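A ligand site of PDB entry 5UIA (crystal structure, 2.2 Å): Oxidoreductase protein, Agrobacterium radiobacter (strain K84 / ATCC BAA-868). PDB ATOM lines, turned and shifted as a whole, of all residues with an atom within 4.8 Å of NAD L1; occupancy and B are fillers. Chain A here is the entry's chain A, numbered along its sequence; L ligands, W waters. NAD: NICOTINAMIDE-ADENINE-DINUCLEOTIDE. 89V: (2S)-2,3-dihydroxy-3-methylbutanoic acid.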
ATOM      1  N   ILE A  11     -25.856   2.861 -14.750  1.00  0.00           N
ATOM      2  CA  ILE A  11     -25.498   3.758 -15.844  1.00  0.00           C
ATOM      3  C   ILE A  11     -24.734   4.965 -15.295  1.00  0.00           C
ATOM      4  O   ILE A  11     -25.265   5.731 -14.494  1.00  0.00           O
ATOM      5  CB  ILE A  11     -26.753   4.264 -16.582  1.00  0.00           C
ATOM      6  CG1 ILE A  11     -27.598   3.089 -17.084  1.00  0.00           C
ATOM      7  CG2 ILE A  11     -26.363   5.186 -17.733  1.00  0.00           C
ATOM      8  CD1 ILE A  11     -29.012   3.476 -17.434  1.00  0.00           C
ATOM      9  N   GLY A  12     -23.503   5.136 -15.782  1.00  0.00           N
ATOM     10  CA  GLY A  12     -22.616   6.226 -15.384  1.00  0.00           C
ATOM     11  C   GLY A  12     -21.534   5.753 -14.415  1.00  0.00           C
ATOM     12  O   GLY A  12     -21.680   5.919 -13.212  1.00  0.00           O
ATOM     13  N   CYS A  13     -20.451   5.199 -14.956  1.00  0.00           N
ATOM     14  CA  CYS A  13     -19.380   4.574 -14.156  1.00  0.00           C
ATOM     15  C   CYS A  13     -18.294   5.549 -13.722  1.00  0.00           C
ATOM     16  O   CYS A  13     -17.098   5.305 -13.923  1.00  0.00           O
ATOM     17  CB  CYS A  13     -18.742   3.432 -14.952  1.00  0.00           C
ATOM     18  SG  CYS A  13     -19.907   2.110 -15.324  1.00  0.00           S
ATOM     19  N   GLY A  14     -18.708   6.647 -13.091  1.00  0.00           N
ATOM     20  CA  GLY A  14     -17.795   7.745 -12.801  1.00  0.00           C
ATOM     21  C   GLY A  14     -17.148   7.695 -11.435  1.00  0.00           C
ATOM     22  O   GLY A  14     -17.022   6.628 -10.842  1.00  0.00           O
ATOM     23  N   PHE A  15     -16.753   8.871 -10.956  1.00  0.00           N
ATOM     24  CA  PHE A  15     -16.057   9.033  -9.686  1.00  0.00           C
ATOM     25  C   PHE A  15     -16.900   8.476  -8.533  1.00  0.00           C
ATOM     26  O   PHE A  15     -16.427   7.603  -7.805  1.00  0.00           O
ATOM     27  CB  PHE A  15     -15.687  10.519  -9.480  1.00  0.00           C
ATOM     28  CG  PHE A  15     -15.383  10.914  -8.058  1.00  0.00           C
ATOM     29  CD1 PHE A  15     -14.103  10.731  -7.521  1.00  0.00           C
ATOM     30  CD2 PHE A  15     -16.362  11.526  -7.260  1.00  0.00           C
ATOM     31  CE1 PHE A  15     -13.808  11.120  -6.206  1.00  0.00           C
ATOM     32  CE2 PHE A  15     -16.078  11.914  -5.954  1.00  0.00           C
ATOM     33  CZ  PHE A  15     -14.798  11.708  -5.425  1.00  0.00           C
ATOM     34  N   PHE A  16     -18.136   8.942  -8.383  1.00  0.00           N
ATOM     35  CA  PHE A  16     -18.993   8.470  -7.283  1.00  0.00           C
ATOM     36  C   PHE A  16     -19.587   7.058  -7.471  1.00  0.00           C
ATOM     37  O   PHE A  16     -19.845   6.366  -6.495  1.00  0.00           O
ATOM     38  CB  PHE A  16     -20.105   9.451  -6.967  1.00  0.00           C
ATOM     39  CG  PHE A  16     -20.611   9.336  -5.546  1.00  0.00           C
ATOM     40  CD1 PHE A  16     -19.833   9.790  -4.477  1.00  0.00           C
ATOM     41  CD2 PHE A  16     -21.851   8.753  -5.275  1.00  0.00           C
ATOM     42  CE1 PHE A  16     -20.301   9.675  -3.168  1.00  0.00           C
ATOM     43  CE2 PHE A  16     -22.308   8.631  -3.968  1.00  0.00           C
ATOM     44  CZ  PHE A  16     -21.535   9.109  -2.920  1.00  0.00           C
ATOM     45  N   ALA A  17     -19.799   6.638  -8.702  1.00  0.00           N
ATOM     46  CA  ALA A  17     -20.353   5.300  -8.990  1.00  0.00           C
ATOM     47  C   ALA A  17     -19.555   4.161  -8.367  1.00  0.00           C
ATOM     48  O   ALA A  17     -20.120   3.122  -8.037  1.00  0.00           O
ATOM     49  CB  ALA A  17     -20.448   5.092 -10.494  1.00  0.00           C
ATOM     50  N   CYS A  36     -22.908   0.569 -17.705  1.00  0.00           N
ATOM     51  CA  CYS A  36     -22.941   1.378 -18.912  1.00  0.00           C
ATOM     52  C   CYS A  36     -22.171   2.691 -18.723  1.00  0.00           C
ATOM     53  O   CYS A  36     -22.323   3.357 -17.703  1.00  0.00           O
ATOM     54  CB  CYS A  36     -24.385   1.657 -19.302  1.00  0.00           C
ATOM     55  SG  CYS A  36     -24.573   2.803 -20.695  1.00  0.00           S
ATOM     56  N   ASP A  37     -21.360   3.072 -19.699  1.00  0.00           N
ATOM     57  CA  ASP A  37     -20.727   4.402 -19.720  1.00  0.00           C
ATOM     58  C   ASP A  37     -20.314   4.754 -21.157  1.00  0.00           C
ATOM     59  O   ASP A  37     -19.781   3.903 -21.876  1.00  0.00           O
ATOM     60  CB  ASP A  37     -19.511   4.431 -18.778  1.00  0.00           C
ATOM     61  CG  ASP A  37     -19.107   5.858 -18.382  1.00  0.00           C
ATOM     62  OD1 ASP A  37     -18.768   6.669 -19.282  1.00  0.00           O
ATOM     63  OD2 ASP A  37     -19.129   6.174 -17.166  1.00  0.00           O
ATOM     64  N   ARG A  38     -20.550   5.995 -21.564  1.00  0.00           N
ATOM     65  CA  ARG A  38     -20.090   6.513 -22.873  1.00  0.00           C
ATOM     66  C   ARG A  38     -18.578   6.497 -23.032  1.00  0.00           C
ATOM     67  O   ARG A  38     -18.080   6.409 -24.150  1.00  0.00           O
ATOM     68  CB  ARG A  38     -20.559   7.953 -23.090  1.00  0.00           C
ATOM     69  CG  ARG A  38     -22.039   8.106 -23.315  1.00  0.00           C
ATOM     70  CD  ARG A  38     -22.407   9.546 -23.596  1.00  0.00           C
ATOM     71  NE  ARG A  38     -23.809   9.669 -23.973  1.00  0.00           N
ATOM     72  CZ  ARG A  38     -24.453  10.829 -24.138  1.00  0.00           C
ATOM     73  NH1 ARG A  38     -23.830  11.986 -23.966  1.00  0.00           N
ATOM     74  NH2 ARG A  38     -25.738  10.810 -24.486  1.00  0.00           N
ATOM     75  N   ASP A  39     -17.868   6.624 -21.909  1.00  0.00           N
ATOM     76  CA  ASP A  39     -16.413   6.641 -21.865  1.00  0.00           C
ATOM     77  C   ASP A  39     -15.920   5.203 -21.705  1.00  0.00           C
ATOM     78  O   ASP A  39     -16.137   4.596 -20.653  1.00  0.00           O
ATOM     79  CB  ASP A  39     -15.969   7.512 -20.689  1.00  0.00           C
ATOM     80  CG  ASP A  39     -14.469   7.738 -20.628  1.00  0.00           C
ATOM     81  OD1 ASP A  39     -13.710   7.016 -21.315  1.00  0.00           O
ATOM     82  OD2 ASP A  39     -14.053   8.648 -19.875  1.00  0.00           O
ATOM     83  N   ARG A  42     -13.660   4.367 -18.562  1.00  0.00           N
ATOM     84  CA  ARG A  42     -14.377   4.159 -17.296  1.00  0.00           C
ATOM     85  C   ARG A  42     -15.120   2.828 -17.257  1.00  0.00           C
ATOM     86  O   ARG A  42     -15.160   2.155 -16.222  1.00  0.00           O
ATOM     87  CB  ARG A  42     -15.369   5.292 -17.034  1.00  0.00           C
ATOM     88  CG  ARG A  42     -14.729   6.663 -16.867  1.00  0.00           C
ATOM     89  CD  ARG A  42     -13.791   6.746 -15.676  1.00  0.00           C
ATOM     90  NE  ARG A  42     -14.448   6.338 -14.426  1.00  0.00           N
ATOM     91  CZ  ARG A  42     -13.832   6.189 -13.254  1.00  0.00           C
ATOM     92  NH1 ARG A  42     -12.525   6.388 -13.143  1.00  0.00           N
ATOM     93  NH2 ARG A  42     -14.525   5.814 -12.189  1.00  0.00           N
ATOM     94  N   ALA A  74     -26.197   7.002 -12.167  1.00  0.00           N
ATOM     95  CA  ALA A  74     -25.135   7.738 -11.512  1.00  0.00           C
ATOM     96  C   ALA A  74     -24.409   8.694 -12.466  1.00  0.00           C
ATOM     97  O   ALA A  74     -23.252   9.064 -12.224  1.00  0.00           O
ATOM     98  CB  ALA A  74     -24.147   6.758 -10.893  1.00  0.00           C
ATOM     99  N   THR A  75     -25.068   9.096 -13.557  1.00  0.00           N
ATOM    100  CA  THR A  75     -24.498  10.078 -14.470  1.00  0.00           C
ATOM    101  C   THR A  75     -24.649  11.482 -13.892  1.00  0.00           C
ATOM    102  O   THR A  75     -25.326  11.686 -12.883  1.00  0.00           O
ATOM    103  CB  THR A  75     -25.176  10.039 -15.853  1.00  0.00           C
ATOM    104  OG1 THR A  75     -26.578  10.307 -15.712  1.00  0.00           O
ATOM    105  CG2 THR A  75     -24.969   8.695 -16.528  1.00  0.00           C
ATOM    106  N   THR A  76     -24.018  12.451 -14.552  1.00  0.00           N
ATOM    107  CA  THR A  76     -24.236  13.875 -14.270  1.00  0.00           C
ATOM    108  C   THR A  76     -25.652  14.282 -14.703  1.00  0.00           C
ATOM    109  O   THR A  76     -26.294  13.575 -15.490  1.00  0.00           O
ATOM    110  CB  THR A  76     -23.201  14.773 -14.979  1.00  0.00           C
ATOM    111  OG1 THR A  76     -23.033  14.333 -16.339  1.00  0.00           O
ATOM    112  CG2 THR A  76     -21.859  14.699 -14.264  1.00  0.00           C
ATOM    113  N   VAL A  77     -26.108  15.423 -14.201  1.00  0.00           N
ATOM    114  CA  VAL A  77     -27.507  15.909 -14.357  1.00  0.00           C
ATOM    115  C   VAL A  77     -28.066  15.957 -15.795  1.00  0.00           C
ATOM    116  O   VAL A  77     -29.256  15.744 -15.968  1.00  0.00           O
ATOM    117  CB  VAL A  77     -27.695  17.299 -13.703  1.00  0.00           C
ATOM    118  CG1 VAL A  77     -26.977  18.394 -14.488  1.00  0.00           C
ATOM    119  CG2 VAL A  77     -29.172  17.643 -13.507  1.00  0.00           C
ATOM    120  N   SER A  79     -28.073  14.033 -18.345  1.00  0.00           N
ATOM    121  CA  SER A  79     -28.721  12.843 -18.898  1.00  0.00           C
ATOM    122  C   SER A  79     -29.817  12.244 -18.018  1.00  0.00           C
ATOM    123  O   SER A  79     -30.402  11.243 -18.397  1.00  0.00           O
ATOM    124  CB  SER A  79     -27.663  11.779 -19.201  1.00  0.00           C
ATOM    125  OG  SER A  79     -27.042  11.363 -17.997  1.00  0.00           O
ATOM    126  N   HIS A  80     -30.119  12.857 -16.871  1.00  0.00           N
ATOM    127  CA  HIS A  80     -31.051  12.242 -15.901  1.00  0.00           C
ATOM    128  C   HIS A  80     -32.462  12.029 -16.419  1.00  0.00           C
ATOM    129  O   HIS A  80     -33.042  10.956 -16.208  1.00  0.00           O
ATOM    130  CB  HIS A  80     -31.144  13.043 -14.597  1.00  0.00           C
ATOM    131  CG  HIS A  80     -29.941  12.937 -13.726  1.00  0.00           C
ATOM    132  ND1 HIS A  80     -29.807  13.670 -12.566  1.00  0.00           N
ATOM    133  CD2 HIS A  80     -28.804  12.225 -13.863  1.00  0.00           C
ATOM    134  CE1 HIS A  80     -28.639  13.380 -12.003  1.00  0.00           C
ATOM    135  NE2 HIS A  80     -28.008  12.514 -12.784  1.00  0.00           N
ATOM    136  N   LEU A  83     -32.685   9.309 -19.148  1.00  0.00           N
ATOM    137  CA  LEU A  83     -32.460   7.966 -18.627  1.00  0.00           C
ATOM    138  C   LEU A  83     -33.629   7.450 -17.780  1.00  0.00           C
ATOM    139  O   LEU A  83     -33.955   6.260 -17.848  1.00  0.00           O
ATOM    140  CB  LEU A  83     -31.138   7.888 -17.862  1.00  0.00           C
ATOM    141  CG  LEU A  83     -29.896   8.007 -18.751  1.00  0.00           C
ATOM    142  CD1 LEU A  83     -28.658   8.152 -17.880  1.00  0.00           C
ATOM    143  CD2 LEU A  83     -29.758   6.823 -19.701  1.00  0.00           C
ATOM    144  N   GLN A  97     -29.362   9.737  -9.340  1.00  0.00           N
ATOM    145  CA  GLN A  97     -28.532  10.622  -8.536  1.00  0.00           C
ATOM    146  C   GLN A  97     -29.070  12.066  -8.514  1.00  0.00           C
ATOM    147  O   GLN A  97     -29.857  12.464  -9.370  1.00  0.00           O
ATOM    148  CB  GLN A  97     -27.051  10.603  -8.998  1.00  0.00           C
ATOM    149  CG  GLN A  97     -26.132   9.691  -8.178  1.00  0.00           C
ATOM    150  CD  GLN A  97     -25.894  10.207  -6.768  1.00  0.00           C
ATOM    151  OE1 GLN A  97     -26.340  11.297  -6.426  1.00  0.00           O
ATOM    152  NE2 GLN A  97     -25.209   9.405  -5.932  1.00  0.00           N
ATOM    153  N   LYS A  98     -28.637  12.807  -7.498  1.00  0.00           N
ATOM    154  CA  LYS A  98     -28.883  14.224  -7.414  1.00  0.00           C
ATOM    155  C   LYS A  98     -27.808  14.963  -8.238  1.00  0.00           C
ATOM    156  O   LYS A  98     -26.818  14.322  -8.640  1.00  0.00           O
ATOM    157  CB  LYS A  98     -28.936  14.736  -5.957  1.00  0.00           C
ATOM    158  CG  LYS A  98     -27.860  14.265  -4.981  1.00  0.00           C
ATOM    159  CD  LYS A  98     -26.426  14.616  -5.351  1.00  0.00           C
ATOM    160  CE  LYS A  98     -26.165  16.110  -5.357  1.00  0.00           C
ATOM    161  NZ  LYS A  98     -24.720  16.404  -5.529  1.00  0.00           N
ATOM    162  N   PRO A  99     -28.006  16.238  -8.572  1.00  0.00           N
ATOM    163  CA  PRO A  99     -29.326  16.894  -8.537  1.00  0.00           C
ATOM    164  C   PRO A  99     -30.333  16.193  -9.462  1.00  0.00           C
ATOM    165  O   PRO A  99     -29.969  15.798 -10.581  1.00  0.00           O
ATOM    166  CB  PRO A  99     -29.025  18.328  -8.983  1.00  0.00           C
ATOM    167  CG  PRO A  99     -27.690  18.294  -9.630  1.00  0.00           C
ATOM    168  CD  PRO A  99     -26.937  17.136  -9.038  1.00  0.00           C
ATOM    169  N   HIS A 124     -31.295   9.319  -5.316  1.00  0.00           N
ATOM    170  CA  HIS A 124     -30.202   8.938  -4.436  1.00  0.00           C
ATOM    171  C   HIS A 124     -29.772  10.197  -3.693  1.00  0.00           C
ATOM    172  O   HIS A 124     -28.859  10.898  -4.123  1.00  0.00           O
ATOM    173  CB  HIS A 124     -29.010   8.323  -5.212  1.00  0.00           C
ATOM    174  CG  HIS A 124     -27.940   7.743  -4.320  1.00  0.00           C
ATOM    175  ND1 HIS A 124     -27.523   6.440  -4.424  1.00  0.00           N
ATOM    176  CD2 HIS A 124     -27.222   8.289  -3.302  1.00  0.00           C
ATOM    177  CE1 HIS A 124     -26.583   6.210  -3.524  1.00  0.00           C
ATOM    178  NE2 HIS A 124     -26.381   7.308  -2.832  1.00  0.00           N
ATOM    179  N   ASN A 126     -28.451  10.934  -0.196  1.00  0.00           N
ATOM    180  CA  ASN A 126     -27.918  10.079   0.878  1.00  0.00           C
ATOM    181  C   ASN A 126     -27.564  10.772   2.213  1.00  0.00           C
ATOM    182  O   ASN A 126     -27.302  10.091   3.212  1.00  0.00           O
ATOM    183  CB  ASN A 126     -26.758   9.180   0.390  1.00  0.00           C
ATOM    184  CG  ASN A 126     -25.584   9.956  -0.213  1.00  0.00           C
ATOM    185  OD1 ASN A 126     -25.286  11.092   0.188  1.00  0.00           O
ATOM    186  ND2 ASN A 126     -24.908   9.332  -1.162  1.00  0.00           N
ATOM    187  N   PHE A 127     -27.592  12.103   2.251  1.00  0.00           N
ATOM    188  CA  PHE A 127     -27.187  12.831   3.464  1.00  0.00           C
ATOM    189  C   PHE A 127     -28.089  12.542   4.658  1.00  0.00           C
ATOM    190  O   PHE A 127     -27.582  12.324   5.748  1.00  0.00           O
ATOM    191  CB  PHE A 127     -27.070  14.343   3.219  1.00  0.00           C
ATOM    192  CG  PHE A 127     -25.695  14.760   2.765  1.00  0.00           C
ATOM    193  CD1 PHE A 127     -25.095  14.156   1.678  1.00  0.00           C
ATOM    194  CD2 PHE A 127     -24.992  15.763   3.450  1.00  0.00           C
ATOM    195  CE1 PHE A 127     -23.820  14.546   1.256  1.00  0.00           C
ATOM    196  CE2 PHE A 127     -23.729  16.156   3.043  1.00  0.00           C
ATOM    197  CZ  PHE A 127     -23.140  15.542   1.937  1.00  0.00           C
ATOM    198  N   GLY A 164     -11.633  15.825  -7.273  1.00  0.00           N
ATOM    199  CA  GLY A 164     -12.451  14.651  -7.526  1.00  0.00           C
ATOM    200  C   GLY A 164     -13.637  14.921  -8.443  1.00  0.00           C
ATOM    201  O   GLY A 164     -14.090  14.012  -9.122  1.00  0.00           O
ATOM    202  N   GLN A 165     -14.128  16.164  -8.446  1.00  0.00           N
ATOM    203  CA  GLN A 165     -15.321  16.563  -9.204  1.00  0.00           C
ATOM    204  C   GLN A 165     -15.078  17.890  -9.976  1.00  0.00           C
ATOM    205  O   GLN A 165     -15.635  18.936  -9.609  1.00  0.00           O
ATOM    206  CB  GLN A 165     -16.524  16.702  -8.237  1.00  0.00           C
ATOM    207  CG  GLN A 165     -16.904  15.403  -7.535  1.00  0.00           C
ATOM    208  CD  GLN A 165     -17.943  15.576  -6.438  1.00  0.00           C
ATOM    209  OE1 GLN A 165     -17.660  15.286  -5.261  1.00  0.00           O
ATOM    210  NE2 GLN A 165     -19.141  16.035  -6.792  1.00  0.00           N
ATOM    211  N   TYR A 167     -16.108  19.288 -12.798  1.00  0.00           N
ATOM    212  CA  TYR A 167     -17.332  19.989 -13.247  1.00  0.00           C
ATOM    213  C   TYR A 167     -17.902  21.047 -12.267  1.00  0.00           C
ATOM    214  O   TYR A 167     -18.513  22.035 -12.704  1.00  0.00           O
ATOM    215  CB  TYR A 167     -18.443  18.988 -13.630  1.00  0.00           C
ATOM    216  CG  TYR A 167     -18.832  18.011 -12.543  1.00  0.00           C
ATOM    217  CD1 TYR A 167     -19.811  18.336 -11.584  1.00  0.00           C
ATOM    218  CD2 TYR A 167     -18.240  16.742 -12.471  1.00  0.00           C
ATOM    219  CE1 TYR A 167     -20.166  17.435 -10.589  1.00  0.00           C
ATOM    220  CE2 TYR A 167     -18.584  15.846 -11.481  1.00  0.00           C
ATOM    221  CZ  TYR A 167     -19.550  16.182 -10.540  1.00  0.00           C
ATOM    222  OH  TYR A 167     -19.889  15.272  -9.555  1.00  0.00           O
ATOM    223  N   ASP A 178     -25.160  21.673  -5.807  1.00  0.00           N
ATOM    224  CA  ASP A 178     -24.319  20.535  -5.446  1.00  0.00           C
ATOM    225  C   ASP A 178     -24.510  20.063  -4.006  1.00  0.00           C
ATOM    226  O   ASP A 178     -24.667  18.860  -3.765  1.00  0.00           O
ATOM    227  CB  ASP A 178     -22.855  20.870  -5.662  1.00  0.00           C
ATOM    228  CG  ASP A 178     -21.945  19.745  -5.264  1.00  0.00           C
ATOM    229  OD1 ASP A 178     -22.167  18.611  -5.722  1.00  0.00           O
ATOM    230  OD2 ASP A 178     -21.009  19.993  -4.465  1.00  0.00           O
ATOM    231  N   HIS A 182     -28.493  18.877  -0.452  1.00  0.00           N
ATOM    232  CA  HIS A 182     -28.460  17.962   0.688  1.00  0.00           C
ATOM    233  C   HIS A 182     -28.910  18.630   1.991  1.00  0.00           C
ATOM    234  O   HIS A 182     -29.696  18.050   2.747  1.00  0.00           O
ATOM    235  CB  HIS A 182     -27.041  17.441   0.930  1.00  0.00           C
ATOM    236  CG  HIS A 182     -26.467  16.645  -0.189  1.00  0.00           C
ATOM    237  ND1 HIS A 182     -27.059  15.488  -0.669  1.00  0.00           N
ATOM    238  CD2 HIS A 182     -25.312  16.794  -0.882  1.00  0.00           C
ATOM    239  CE1 HIS A 182     -26.310  14.983  -1.625  1.00  0.00           C
ATOM    240  NE2 HIS A 182     -25.247  15.752  -1.777  1.00  0.00           N
ATOM    241  N   ILE A 291     -20.321   9.491   4.255  1.00  0.00           N
ATOM    242  CA  ILE A 291     -21.088   9.504   3.022  1.00  0.00           C
ATOM    243  C   ILE A 291     -21.163   8.087   2.453  1.00  0.00           C
ATOM    244  O   ILE A 291     -22.230   7.633   2.004  1.00  0.00           O
ATOM    245  CB  ILE A 291     -20.475  10.489   1.976  1.00  0.00           C
ATOM    246  CG1 ILE A 291     -20.674  11.933   2.446  1.00  0.00           C
ATOM    247  CG2 ILE A 291     -21.087  10.296   0.585  1.00  0.00           C
ATOM    248  CD1 ILE A 291     -19.932  12.975   1.613  1.00  0.00           C
HETATM  249  PA  NAD L   1     -18.346  11.951 -13.124  1.00  0.00           P
HETATM  250  O1A NAD L   1     -18.220  12.932 -14.272  1.00  0.00           O
HETATM  251  O2A NAD L   1     -17.118  11.459 -12.398  1.00  0.00           O
HETATM  252  O5B NAD L   1     -19.129  10.647 -13.655  1.00  0.00           O
HETATM  253  C5B NAD L   1     -20.176  10.681 -14.621  1.00  0.00           C
HETATM  254  C4B NAD L   1     -19.962   9.522 -15.582  1.00  0.00           C
HETATM  255  O4B NAD L   1     -21.135   9.305 -16.364  1.00  0.00           O
HETATM  256  C3B NAD L   1     -18.819   9.764 -16.558  1.00  0.00           C
HETATM  257  O3B NAD L   1     -17.911   8.649 -16.494  1.00  0.00           O
HETATM  258  C2B NAD L   1     -19.459   9.877 -17.931  1.00  0.00           C
HETATM  259  O2B NAD L   1     -18.676   9.251 -18.952  1.00  0.00           O
HETATM  260  C1B NAD L   1     -20.792   9.173 -17.743  1.00  0.00           C
HETATM  261  N9A NAD L   1     -21.949   9.646 -18.526  1.00  0.00           N
HETATM  262  C8A NAD L   1     -22.406  10.905 -18.672  1.00  0.00           C
HETATM  263  N7A NAD L   1     -23.534  10.921 -19.429  1.00  0.00           N
HETATM  264  C5A NAD L   1     -23.814   9.644 -19.775  1.00  0.00           C
HETATM  265  C6A NAD L   1     -24.842   8.924 -20.573  1.00  0.00           C
HETATM  266  N6A NAD L   1     -25.855   9.580 -21.195  1.00  0.00           N
HETATM  267  N1A NAD L   1     -24.756   7.581 -20.666  1.00  0.00           N
HETATM  268  C2A NAD L   1     -23.767   6.877 -20.077  1.00  0.00           C
HETATM  269  N3A NAD L   1     -22.792   7.464 -19.343  1.00  0.00           N
HETATM  270  C4A NAD L   1     -22.771   8.811 -19.170  1.00  0.00           C
HETATM  271  O3  NAD L   1     -19.383  12.591 -12.070  1.00  0.00           O
HETATM  272  PN  NAD L   1     -19.473  12.133 -10.531  1.00  0.00           P
HETATM  273  O1N NAD L   1     -18.550  13.015  -9.732  1.00  0.00           O
HETATM  274  O2N NAD L   1     -19.338  10.633 -10.415  1.00  0.00           O
HETATM  275  O5D NAD L   1     -20.986  12.556 -10.189  1.00  0.00           O
HETATM  276  C5D NAD L   1     -22.087  11.914 -10.804  1.00  0.00           C
HETATM  277  C4D NAD L   1     -23.374  12.344 -10.112  1.00  0.00           C
HETATM  278  O4D NAD L   1     -23.324  11.946  -8.735  1.00  0.00           O
HETATM  279  C3D NAD L   1     -23.562  13.853 -10.144  1.00  0.00           C
HETATM  280  O3D NAD L   1     -24.907  14.160 -10.565  1.00  0.00           O
HETATM  281  C2D NAD L   1     -23.274  14.327  -8.725  1.00  0.00           C
HETATM  282  O2D NAD L   1     -24.103  15.415  -8.330  1.00  0.00           O
HETATM  283  C1D NAD L   1     -23.558  13.086  -7.886  1.00  0.00           C
HETATM  284  N1N NAD L   1     -22.759  12.920  -6.662  1.00  0.00           N
HETATM  285  C2N NAD L   1     -23.424  12.531  -5.548  1.00  0.00           C
HETATM  286  C3N NAD L   1     -22.782  12.331  -4.333  1.00  0.00           C
HETATM  287  C7N NAD L   1     -23.589  11.889  -3.139  1.00  0.00           C
HETATM  288  O7N NAD L   1     -24.566  11.180  -3.315  1.00  0.00           O
HETATM  289  N7N NAD L   1     -23.258  12.251  -1.893  1.00  0.00           N
HETATM  290  C4N NAD L   1     -21.398  12.545  -4.281  1.00  0.00           C
HETATM  291  C5N NAD L   1     -20.720  12.936  -5.424  1.00  0.00           C
HETATM  292  C6N NAD L   1     -21.421  13.119  -6.616  1.00  0.00           C
HETATM  293  OXT 89V L   2     -23.057  15.792  -3.380  1.00  0.00           O
HETATM  294  C   89V L   2     -22.026  15.419  -2.776  1.00  0.00           C
HETATM  295  O   89V L   2     -22.060  14.607  -1.835  1.00  0.00           O
HETATM  296  CA  89V L   2     -20.678  15.923  -3.230  1.00  0.00           C
HETATM  297  CB  89V L   2     -20.040  16.950  -2.269  1.00  0.00           C
HETATM  298  CG2 89V L   2     -18.554  17.067  -2.616  1.00  0.00           C
HETATM  299  CG1 89V L   2     -20.188  16.637  -0.779  1.00  0.00           C
HETATM  300  O1  89V L   2     -20.611  18.248  -2.458  1.00  0.00           O
HETATM  301  O2  89V L   2     -20.801  16.485  -4.544  1.00  0.00           O
HETATM  302  O   HOH W   1     -20.504   8.288 -11.355  1.00  0.00           O
HETATM  303  O   HOH W   2     -23.110  18.080  -8.147  1.00  0.00           O
HETATM  304  O   HOH W   3     -15.684  13.739 -11.381  1.00  0.00           O
HETATM  305  O   HOH W   4     -24.958  13.181 -18.263  1.00  0.00           O
HETATM  306  O   HOH W   5     -24.433  16.777 -12.266  1.00  0.00           O
HETATM  307  O   HOH W   6     -15.678   9.909 -18.186  1.00  0.00           O
HETATM  308  O   HOH W   7     -26.084   6.190 -22.863  1.00  0.00           O
HETATM  309  O   HOH W   8     -26.943  11.842  -2.468  1.00  0.00           O
HETATM  310  O   HOH W   9     -28.240   7.846 -22.878  1.00  0.00           O
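Water W8 lies within hydrogen-bond range of an oxygen (O7N) of NAD L1 (2.6 Å), the backbone carbonyl oxygen of His 124 (2.7 Å) and the backbone NH of Asn 126 (2.9 Å).
Water W1 lies within hydrogen-bond range of an oxygen (O2N) of NAD L1 (2.8 Å), the backbone carbonyl oxygen of Ala 74 (3.0 Å), the backbone NH of Gly 14 (3.0 Å), the backbone NH of Ala 17 (3.2 Å) and the backbone carbonyl oxygen of Gly 12 (3.2 Å).
Water W2 bridges OD1 of Asp 178 (2.7 Å) and O2D of NAD L1 (2.8 Å).
Water W4 lies within hydrogen-bond range of the side-chain hydroxyl (OG) of Ser 79 (2.8 Å), a nitrogen (N7A) of NAD L1 (2.9 Å) and the side-chain hydroxyl (OG1) of Thr 76 (3.0 Å).
Water W6 bridges the side-chain carboxylate (OD2) of Asp 39 (2.7 Å) and an oxygen (O3B) of NAD L1 (3.1 Å).
Water W5 bridges N of Val 77 and O3D of NAD L1.
O of Thr 75 lies within hydrogen-bond range of O3D of NAD L1.
N of Arg 38 is in hydrogen-bond range of N3A of NAD L1 (3.5 Å).
O2N of NAD L1 is in hydrogen-bond range of N of Phe 16 (2.9 Å).
An oxygen (O1) of 89V L2 sits at hydrogen-bond distance from the side-chain carboxylate of Asp 178 (2.7 Å).
ND2 of Asn 126 is in hydrogen-bond range of O7N of NAD L1 (2.9 Å).
OXT of 89V L2 is in hydrogen-bond range of NE2 of His 182 (2.7 Å).
The side-chain hydroxyl of Tyr 167 is in hydrogen-bond range of an oxygen (O1N) of NAD L1, 2.6 Å away.
OXT of 89V L2 is in salt-bridge range of NZ of Lys 98, 2.8 Å away.
The side-chain amide nitrogen (NE2) of Gln 97 sits at hydrogen-bond distance from an oxygen (O7N) of NAD L1 (3.2 Å).
NE2 of Gln 165 sits at hydrogen-bond distance from O2 of 89V L2 (2.8 Å).
The backbone NH (N) of Phe 15 is in hydrogen-bond range of an oxygen (O2A) of NAD L1 (3.0 Å).
The backbone carbonyl oxygen (O) of Lys 98 is in hydrogen-bond range of an oxygen (O3D) of NAD L1 (2.7 Å).
The side-chain amino group of Lys 98 is in hydrogen-bond range of an oxygen (O2D) of NAD L1, at 3.0 Å.
OD1 of Asp 37 is in hydrogen-bond range of O2B of NAD L1 (2.6 Å).
The side-chain carboxylate (OD1) of Asp 37 lies within hydrogen-bond range of the backbone NH (N) of Asp 39, 2.8 Å away.
The guanidinium group (NE) of Arg 42 lies within hydrogen-bond range of the backbone carbonyl oxygen (O) of Cys 13 (2.9 Å).
The side-chain hydroxyl (OG) of Ser 79 is in hydrogen-bond range of the backbone carbonyl oxygen (O) of Thr 76, 3.4 Å away.
O of Gly 14 lies within hydrogen-bond range of NH2 of Arg 42 (3.0 Å).
The backbone carbonyl oxygen of Cys 36 is in hydrogen-bond range of the backbone NH of Gly 12 (2.9 Å).
OD2 of Asp 37 is in hydrogen-bond range of N of Cys 13, 2.8 Å away.
OH of Tyr 167 sits at hydrogen-bond distance from NE2 of Gln 165.
The backbone carbonyl oxygen (O) of Thr 76 sits close to a ring nitrogen (NE2) of His 80 (3.4 Å).
Merely in contact with NAD L1: Gly 14 (3.3 Å), Pro 99 (3.4 Å), Ala 74 (3.4 Å), Ser 79 (3.5 Å), Gly 12 (3.6 Å), Gln 165 (3.6 Å), Asp 39 (3.7 Å), Arg 42 (3.8 Å), Thr 76 (3.8 Å), Ile 291 (3.8 Å), Ile 11 (3.9 Å), His 124 (3.9 Å) and Phe 127 (3.9 Å).
Within 4 Å of NAD L1: Ile 11, Gly 12, Gly 14, Phe 15, Phe 16, Asp 37, Arg 38, Asp 39, Arg 42, Ala 74, Thr 75, Thr 76, Ser 79, Gln 97, Lys 98, Pro 99, His 124, Asn 126, Phe 127, Gln 165, Tyr 167 and Ile 291.
A nitrogen (N7N) of NAD L1 is in hydrogen-bond range of an oxygen (O) of 89V L2 (2.6 Å).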
